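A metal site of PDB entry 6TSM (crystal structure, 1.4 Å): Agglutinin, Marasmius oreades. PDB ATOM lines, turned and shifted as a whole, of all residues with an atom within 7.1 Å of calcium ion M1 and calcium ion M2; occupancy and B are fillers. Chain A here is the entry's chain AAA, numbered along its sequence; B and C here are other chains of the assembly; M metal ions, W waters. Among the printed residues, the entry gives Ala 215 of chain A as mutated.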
ATOM      1  N   ARG A 209     -10.623  -3.135   1.115  1.00  0.00           N
ATOM      2  CA  ARG A 209      -9.789  -2.840   2.292  1.00  0.00           C
ATOM      3  C   ARG A 209     -10.672  -2.885   3.531  1.00  0.00           C
ATOM      4  O   ARG A 209     -11.741  -2.249   3.516  1.00  0.00           O
ATOM      5  CB  ARG A 209      -9.142  -1.474   2.144  1.00  0.00           C
ATOM      6  CG  ARG A 209      -8.148  -1.399   0.980  1.00  0.00           C
ATOM      7  CD  ARG A 209      -7.669   0.022   0.734  1.00  0.00           C
ATOM      8  NE  ARG A 209      -7.011   0.565   1.898  1.00  0.00           N
ATOM      9  CZ  ARG A 209      -6.714   1.845   2.073  1.00  0.00           C
ATOM     10  NH1 ARG A 209      -6.919   2.719   1.118  1.00  0.00           N
ATOM     11  NH2 ARG A 209      -6.193   2.236   3.232  1.00  0.00           N
ATOM     12  N   GLU A 210     -10.188  -3.505   4.585  1.00  0.00           N
ATOM     13  CA  GLU A 210     -10.965  -3.754   5.822  1.00  0.00           C
ATOM     14  C   GLU A 210     -11.491  -2.419   6.367  1.00  0.00           C
ATOM     15  O   GLU A 210     -10.642  -1.536   6.670  1.00  0.00           O
ATOM     16  CB  GLU A 210     -10.059  -4.464   6.838  1.00  0.00           C
ATOM     17  CG  GLU A 210     -10.710  -4.734   8.181  1.00  0.00           C
ATOM     18  CD  GLU A 210      -9.725  -5.268   9.237  1.00  0.00           C
ATOM     19  OE1 GLU A 210      -8.595  -5.659   8.849  1.00  0.00           O
ATOM     20  OE2 GLU A 210     -10.042  -5.200  10.421  1.00  0.00           O
ATOM     21  N   GLN A 211     -12.828  -2.271   6.420  1.00  0.00           N
ATOM     22  CA  GLN A 211     -13.619  -1.087   6.951  1.00  0.00           C
ATOM     23  C   GLN A 211     -13.449   0.164   6.051  1.00  0.00           C
ATOM     24  O   GLN A 211     -14.447   0.854   5.826  1.00  0.00           O
ATOM     25  CB  GLN A 211     -13.249  -0.789   8.416  1.00  0.00           C
ATOM     26  CG  GLN A 211     -13.711  -1.882   9.379  1.00  0.00           C
ATOM     27  CD  GLN A 211     -13.828  -1.398  10.810  1.00  0.00           C
ATOM     28  OE1 GLN A 211     -14.402  -0.350  11.084  1.00  0.00           O
ATOM     29  NE2 GLN A 211     -13.285  -2.157  11.724  1.00  0.00           N
ATOM     30  N   ILE A 212     -12.234   0.481   5.622  1.00  0.00           N
ATOM     31  CA  ILE A 212     -11.941   1.809   5.003  1.00  0.00           C
ATOM     32  C   ILE A 212     -12.419   1.819   3.509  1.00  0.00           C
ATOM     33  O   ILE A 212     -12.736   2.905   3.005  1.00  0.00           O
ATOM     34  CB  ILE A 212     -10.443   2.153   5.139  1.00  0.00           C
ATOM     35  CG1 ILE A 212     -10.167   3.632   4.794  1.00  0.00           C
ATOM     36  CG2 ILE A 212      -9.569   1.217   4.329  1.00  0.00           C
ATOM     37  CD1 ILE A 212     -10.803   4.617   5.733  1.00  0.00           C
ATOM     38  N   TYR A 213     -12.486   0.674   2.880  1.00  0.00           N
ATOM     39  CA  TYR A 213     -13.186   0.577   1.543  1.00  0.00           C
ATOM     40  C   TYR A 213     -13.650  -0.834   1.327  1.00  0.00           C
ATOM     41  O   TYR A 213     -12.997  -1.610   0.591  1.00  0.00           O
ATOM     42  CB  TYR A 213     -12.272   1.062   0.400  1.00  0.00           C
ATOM     43  CG  TYR A 213     -13.007   1.799  -0.673  1.00  0.00           C
ATOM     44  CD1 TYR A 213     -13.492   3.067  -0.432  1.00  0.00           C
ATOM     45  CD2 TYR A 213     -13.429   1.154  -1.825  1.00  0.00           C
ATOM     46  CE1 TYR A 213     -14.242   3.741  -1.384  1.00  0.00           C
ATOM     47  CE2 TYR A 213     -14.225   1.803  -2.761  1.00  0.00           C
ATOM     48  CZ  TYR A 213     -14.615   3.110  -2.538  1.00  0.00           C
ATOM     49  OH  TYR A 213     -15.392   3.770  -3.479  1.00  0.00           O
ATOM     50  N   ASP A 214     -14.667  -1.206   2.063  1.00  0.00           N
ATOM     51  CA  ASP A 214     -15.184  -2.582   2.054  1.00  0.00           C
ATOM     52  C   ASP A 214     -16.581  -2.568   1.374  1.00  0.00           C
ATOM     53  O   ASP A 214     -16.875  -1.623   0.642  1.00  0.00           O
ATOM     54  CB  ASP A 214     -15.164  -3.170   3.465  1.00  0.00           C
ATOM     55  CG  ASP A 214     -16.063  -2.466   4.468  1.00  0.00           C
ATOM     56  OD1 ASP A 214     -16.315  -1.291   4.286  1.00  0.00           O
ATOM     57  OD2 ASP A 214     -16.420  -3.110   5.482  1.00  0.00           O
ATOM     58  N   ALA A 215     -17.377  -3.597   1.565  1.00  0.00           N
ATOM     59  CA  ALA A 215     -18.594  -3.792   0.716  1.00  0.00           C
ATOM     60  C   ALA A 215     -19.489  -2.535   0.763  1.00  0.00           C
ATOM     61  O   ALA A 215     -20.046  -2.158  -0.303  1.00  0.00           O
ATOM     62  CB  ALA A 215     -19.364  -5.043   1.161  1.00  0.00           C
ATOM     63  N   ASP A 216     -19.688  -1.938   1.938  1.00  0.00           N
ATOM     64  CA  ASP A 216     -20.628  -0.813   2.059  1.00  0.00           C
ATOM     65  C   ASP A 216     -20.079   0.385   1.229  1.00  0.00           C
ATOM     66  O   ASP A 216     -20.880   1.075   0.604  1.00  0.00           O
ATOM     67  CB  ASP A 216     -20.891  -0.443   3.532  1.00  0.00           C
ATOM     68  CG  ASP A 216     -19.651  -0.383   4.381  1.00  0.00           C
ATOM     69  OD1 ASP A 216     -19.015   0.669   4.403  1.00  0.00           O
ATOM     70  OD2 ASP A 216     -19.295  -1.408   4.951  1.00  0.00           O
ATOM     71  N   ASP A 217     -18.777   0.529   1.136  1.00  0.00           N
ATOM     72  CA  ASP A 217     -18.187   1.652   0.364  1.00  0.00           C
ATOM     73  C   ASP A 217     -18.442   1.418  -1.129  1.00  0.00           C
ATOM     74  O   ASP A 217     -18.816   2.387  -1.835  1.00  0.00           O
ATOM     75  CB  ASP A 217     -16.719   1.808   0.670  1.00  0.00           C
ATOM     76  CG  ASP A 217     -16.458   2.162   2.134  1.00  0.00           C
ATOM     77  OD1 ASP A 217     -16.761   3.311   2.509  1.00  0.00           O
ATOM     78  OD2 ASP A 217     -16.208   1.247   2.902  1.00  0.00           O
ATOM     79  N   PHE A 218     -18.259   0.200  -1.598  1.00  0.00           N
ATOM     80  CA  PHE A 218     -18.495  -0.130  -3.037  1.00  0.00           C
ATOM     81  C   PHE A 218     -19.969   0.124  -3.402  1.00  0.00           C
ATOM     82  O   PHE A 218     -20.242   0.728  -4.415  1.00  0.00           O
ATOM     83  CB  PHE A 218     -18.093  -1.562  -3.345  1.00  0.00           C
ATOM     84  CG  PHE A 218     -16.620  -1.786  -3.526  1.00  0.00           C
ATOM     85  CD1 PHE A 218     -15.798  -2.001  -2.437  1.00  0.00           C
ATOM     86  CD2 PHE A 218     -16.061  -1.820  -4.796  1.00  0.00           C
ATOM     87  CE1 PHE A 218     -14.453  -2.306  -2.600  1.00  0.00           C
ATOM     88  CE2 PHE A 218     -14.709  -2.075  -4.967  1.00  0.00           C
ATOM     89  CZ  PHE A 218     -13.914  -2.318  -3.863  1.00  0.00           C
ATOM     90  N   VAL B   2     -20.946  -8.106  10.987  1.00  0.00           N
ATOM     91  CA  VAL B   2     -20.675  -6.720  10.494  1.00  0.00           C
ATOM     92  C   VAL B   2     -20.693  -6.734   8.950  1.00  0.00           C
ATOM     93  O   VAL B   2     -20.335  -7.781   8.362  1.00  0.00           O
ATOM     94  CB  VAL B   2     -19.348  -6.170  11.049  1.00  0.00           C
ATOM     95  CG1 VAL B   2     -19.395  -6.007  12.556  1.00  0.00           C
ATOM     96  CG2 VAL B   2     -18.150  -7.022  10.627  1.00  0.00           C
ATOM     97  N   VAL B   3     -21.235  -5.670   8.350  1.00  0.00           N
ATOM     98  CA  VAL B   3     -21.320  -5.508   6.865  1.00  0.00           C
ATOM     99  C   VAL B   3     -19.907  -5.371   6.308  1.00  0.00           C
ATOM    100  O   VAL B   3     -19.241  -4.372   6.633  1.00  0.00           O
ATOM    101  CB  VAL B   3     -22.174  -4.286   6.482  1.00  0.00           C
ATOM    102  CG1 VAL B   3     -22.093  -3.979   4.996  1.00  0.00           C
ATOM    103  CG2 VAL B   3     -23.633  -4.471   6.909  1.00  0.00           C
ATOM    104  N   ARG B   4     -19.443  -6.383   5.567  1.00  0.00           N
ATOM    105  CA  ARG B   4     -17.997  -6.538   5.193  1.00  0.00           C
ATOM    106  C   ARG B   4     -17.884  -6.815   3.699  1.00  0.00           C
ATOM    107  O   ARG B   4     -16.974  -6.292   3.059  1.00  0.00           O
ATOM    108  CB  ARG B   4     -17.365  -7.683   5.982  1.00  0.00           C
ATOM    109  CG  ARG B   4     -16.958  -7.304   7.395  1.00  0.00           C
ATOM    110  CD  ARG B   4     -16.131  -8.393   8.062  1.00  0.00           C
ATOM    111  NE  ARG B   4     -14.793  -8.520   7.477  1.00  0.00           N
ATOM    112  CZ  ARG B   4     -14.401  -9.523   6.697  1.00  0.00           C
ATOM    113  NH1 ARG B   4     -15.239 -10.500   6.376  1.00  0.00           N
ATOM    114  NH2 ARG B   4     -13.162  -9.554   6.244  1.00  0.00           N
ATOM    115  OXT ARG B   4     -18.685  -7.638   3.099  1.00  0.00           O
ATOM    116  N   ILE C 181     -25.794   0.074  11.042  1.00  0.00           N
ATOM    117  CA  ILE C 181     -24.345   0.261  11.250  1.00  0.00           C
ATOM    118  C   ILE C 181     -23.575  -0.492  10.139  1.00  0.00           C
ATOM    119  O   ILE C 181     -23.915  -1.651   9.868  1.00  0.00           O
ATOM    120  CB  ILE C 181     -23.944  -0.237  12.647  1.00  0.00           C
ATOM    121  CG1 ILE C 181     -24.593   0.627  13.736  1.00  0.00           C
ATOM    122  CG2 ILE C 181     -22.455  -0.295  12.787  1.00  0.00           C
ATOM    123  CD1 ILE C 181     -24.481   0.057  15.113  1.00  0.00           C
ATOM    124  N   LEU C 182     -22.524   0.132   9.606  1.00  0.00           N
ATOM    125  CA  LEU C 182     -21.810  -0.417   8.422  1.00  0.00           C
ATOM    126  C   LEU C 182     -20.387  -0.871   8.811  1.00  0.00           C
ATOM    127  O   LEU C 182     -19.824  -1.752   8.071  1.00  0.00           O
ATOM    128  CB  LEU C 182     -21.766   0.645   7.328  1.00  0.00           C
ATOM    129  CG  LEU C 182     -23.122   1.121   6.832  1.00  0.00           C
ATOM    130  CD1 LEU C 182     -22.954   2.222   5.800  1.00  0.00           C
ATOM    131  CD2 LEU C 182     -23.927  -0.022   6.245  1.00  0.00           C
ATOM    132  N   ASP C 183     -19.771  -0.225   9.820  1.00  0.00           N
ATOM    133  CA  ASP C 183     -18.344  -0.447  10.172  1.00  0.00           C
ATOM    134  C   ASP C 183     -18.205  -0.448  11.708  1.00  0.00           C
ATOM    135  O   ASP C 183     -19.250  -0.444  12.385  1.00  0.00           O
ATOM    136  CB  ASP C 183     -17.443   0.617   9.522  1.00  0.00           C
ATOM    137  CG  ASP C 183     -17.429   0.575   7.977  1.00  0.00           C
ATOM    138  OD1 ASP C 183     -17.090  -0.462   7.424  1.00  0.00           O
ATOM    139  OD2 ASP C 183     -17.717   1.616   7.363  1.00  0.00           O
ATOM    140  N   GLY C 184     -16.999  -0.605  12.202  1.00  0.00           N
ATOM    141  CA  GLY C 184     -16.753  -0.893  13.634  1.00  0.00           C
ATOM    142  C   GLY C 184     -16.146   0.315  14.371  1.00  0.00           C
ATOM    143  O   GLY C 184     -16.340   0.401  15.588  1.00  0.00           O
ATOM    144  N   TYR C 186     -14.485   4.377  13.812  1.00  0.00           N
ATOM    145  CA  TYR C 186     -14.599   5.546  12.890  1.00  0.00           C
ATOM    146  C   TYR C 186     -13.668   6.664  13.354  1.00  0.00           C
ATOM    147  O   TYR C 186     -13.883   7.201  14.457  1.00  0.00           O
ATOM    148  CB  TYR C 186     -16.016   6.056  12.851  1.00  0.00           C
ATOM    149  CG  TYR C 186     -17.033   5.063  12.373  1.00  0.00           C
ATOM    150  CD1 TYR C 186     -17.685   4.216  13.258  1.00  0.00           C
ATOM    151  CD2 TYR C 186     -17.406   5.014  11.050  1.00  0.00           C
ATOM    152  CE1 TYR C 186     -18.723   3.401  12.843  1.00  0.00           C
ATOM    153  CE2 TYR C 186     -18.411   4.173  10.606  1.00  0.00           C
ATOM    154  CZ  TYR C 186     -19.061   3.348  11.508  1.00  0.00           C
ATOM    155  OH  TYR C 186     -20.079   2.545  11.074  1.00  0.00           O
ATOM    156  N   LYS C 223     -21.743  11.142   1.467  1.00  0.00           N
ATOM    157  CA  LYS C 223     -21.209   9.945   2.115  1.00  0.00           C
ATOM    158  C   LYS C 223     -20.184   9.258   1.180  1.00  0.00           C
ATOM    159  O   LYS C 223     -19.158   8.835   1.659  1.00  0.00           O
ATOM    160  CB  LYS C 223     -22.318   8.963   2.482  1.00  0.00           C
ATOM    161  CG  LYS C 223     -21.819   7.699   3.163  1.00  0.00           C
ATOM    162  CD  LYS C 223     -22.712   7.172   4.253  1.00  0.00           C
ATOM    163  CE  LYS C 223     -22.159   5.916   4.918  1.00  0.00           C
ATOM    164  NZ  LYS C 223     -20.796   6.121   5.478  1.00  0.00           N
ATOM    165  N   PHE C 239     -10.369   0.627   9.913  1.00  0.00           N
ATOM    166  CA  PHE C 239     -11.191   1.740  10.412  1.00  0.00           C
ATOM    167  C   PHE C 239     -11.946   2.384   9.243  1.00  0.00           C
ATOM    168  O   PHE C 239     -11.568   2.119   8.075  1.00  0.00           O
ATOM    169  CB  PHE C 239     -10.326   2.769  11.119  1.00  0.00           C
ATOM    170  CG  PHE C 239      -9.447   3.549  10.178  1.00  0.00           C
ATOM    171  CD1 PHE C 239      -8.310   2.972   9.612  1.00  0.00           C
ATOM    172  CD2 PHE C 239      -9.768   4.837   9.819  1.00  0.00           C
ATOM    173  CE1 PHE C 239      -7.565   3.670   8.667  1.00  0.00           C
ATOM    174  CE2 PHE C 239      -9.001   5.533   8.896  1.00  0.00           C
ATOM    175  CZ  PHE C 239      -7.918   4.939   8.325  1.00  0.00           C
ATOM    176  N   ALA C 240     -12.951   3.187   9.551  1.00  0.00           N
ATOM    177  CA  ALA C 240     -13.682   3.988   8.558  1.00  0.00           C
ATOM    178  C   ALA C 240     -13.707   5.452   8.988  1.00  0.00           C
ATOM    179  O   ALA C 240     -13.171   5.754  10.074  1.00  0.00           O
ATOM    180  CB  ALA C 240     -15.095   3.442   8.397  1.00  0.00           C
ATOM    181  N   ILE C 241     -14.192   6.317   8.127  1.00  0.00           N
ATOM    182  CA  ILE C 241     -14.395   7.751   8.442  1.00  0.00           C
ATOM    183  C   ILE C 241     -15.854   7.944   8.827  1.00  0.00           C
ATOM    184  O   ILE C 241     -16.732   7.455   8.089  1.00  0.00           O
ATOM    185  CB  ILE C 241     -13.994   8.649   7.239  1.00  0.00           C
ATOM    186  CG1 ILE C 241     -12.664   8.225   6.612  1.00  0.00           C
ATOM    187  CG2 ILE C 241     -13.979  10.101   7.657  1.00  0.00           C
ATOM    188  CD1 ILE C 241     -11.510   8.163   7.562  1.00  0.00           C
ATOM    189  N   TYR C 293     -24.633   4.490   8.642  1.00  0.00           N
ATOM    190  CA  TYR C 293     -23.328   5.099   9.002  1.00  0.00           C
ATOM    191  C   TYR C 293     -22.347   4.010   9.287  1.00  0.00           C
ATOM    192  O   TYR C 293     -21.164   4.188   9.104  1.00  0.00           O
ATOM    193  CB  TYR C 293     -23.483   6.036  10.205  1.00  0.00           C
ATOM    194  CG  TYR C 293     -24.059   5.372  11.437  1.00  0.00           C
ATOM    195  CD1 TYR C 293     -25.421   5.301  11.641  1.00  0.00           C
ATOM    196  CD2 TYR C 293     -23.230   4.916  12.455  1.00  0.00           C
ATOM    197  CE1 TYR C 293     -25.966   4.750  12.803  1.00  0.00           C
ATOM    198  CE2 TYR C 293     -23.744   4.325  13.607  1.00  0.00           C
ATOM    199  CZ  TYR C 293     -25.120   4.282  13.799  1.00  0.00           C
ATOM    200  OH  TYR C 293     -25.654   3.715  14.946  1.00  0.00           O
ATOM    201  OXT TYR C 293     -22.741   2.893   9.709  1.00  0.00           O
HETATM  202 CA    CA M   1     -16.739   0.829   5.214  1.00  0.00          CA
HETATM  203 CA    CA M   2     -18.247  -2.498   6.711  1.00  0.00          CA
HETATM  204  O   HOH W   1     -17.061  -3.629   8.625  1.00  0.00           O
HETATM  205  O   HOH W   2     -16.724   3.232   5.078  1.00  0.00           O
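The side-chain hydroxyl (OH) of Tyr 186 of chain C is in hydrogen-bond range of the backbone NH (N) of Asp 183 of chain C, 3.1 Å away. N of Leu 182 of chain C is in hydrogen-bond range of OXT of Tyr 293 of chain C, 2.8 Å away. The side-chain amide oxygen (OE1) of Gln 211 lies within hydrogen-bond range of the backbone NH (N) of Gly 184 of chain C (2.8 Å). The backbone carbonyl oxygen of Arg 209 lies within hydrogen-bond range of the backbone NH of Asp 214.
Within 4 Å of calcium ion M2: Asp 214, Asp 216, Val 3 of chain B, Leu 182 of chain C and Asp 183 of chain C.
Calcium ion M1 is bound by the side-chain carboxylate (OD1) of Asp 214 (2.4 Å), the backbone carbonyl oxygen (O) of Gln 211 (2.4 Å), water W2 (2.4 Å), the side-chain carboxylate (OD2) of Asp 217 (2.4 Å), the side-chain carboxylate (OD1) of Asp 216 (2.4 Å), the side-chain carboxylate (OD2) of Asp 183 of chain C (2.5 Å) and the side-chain carboxylate (OD1) of Asp 183 of chain C (2.6 Å). Calcium ion M1 has seven donor atoms within binding distance.
Calcium ion M2 is bound by O of Val 3 of chain B, O of Leu 182 of chain C, OD2 of Asp 214, OD2 of Asp 216, OD1 of Asp 183 of chain C and water W1. Calcium ion M2 has six donor atoms within binding distance.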
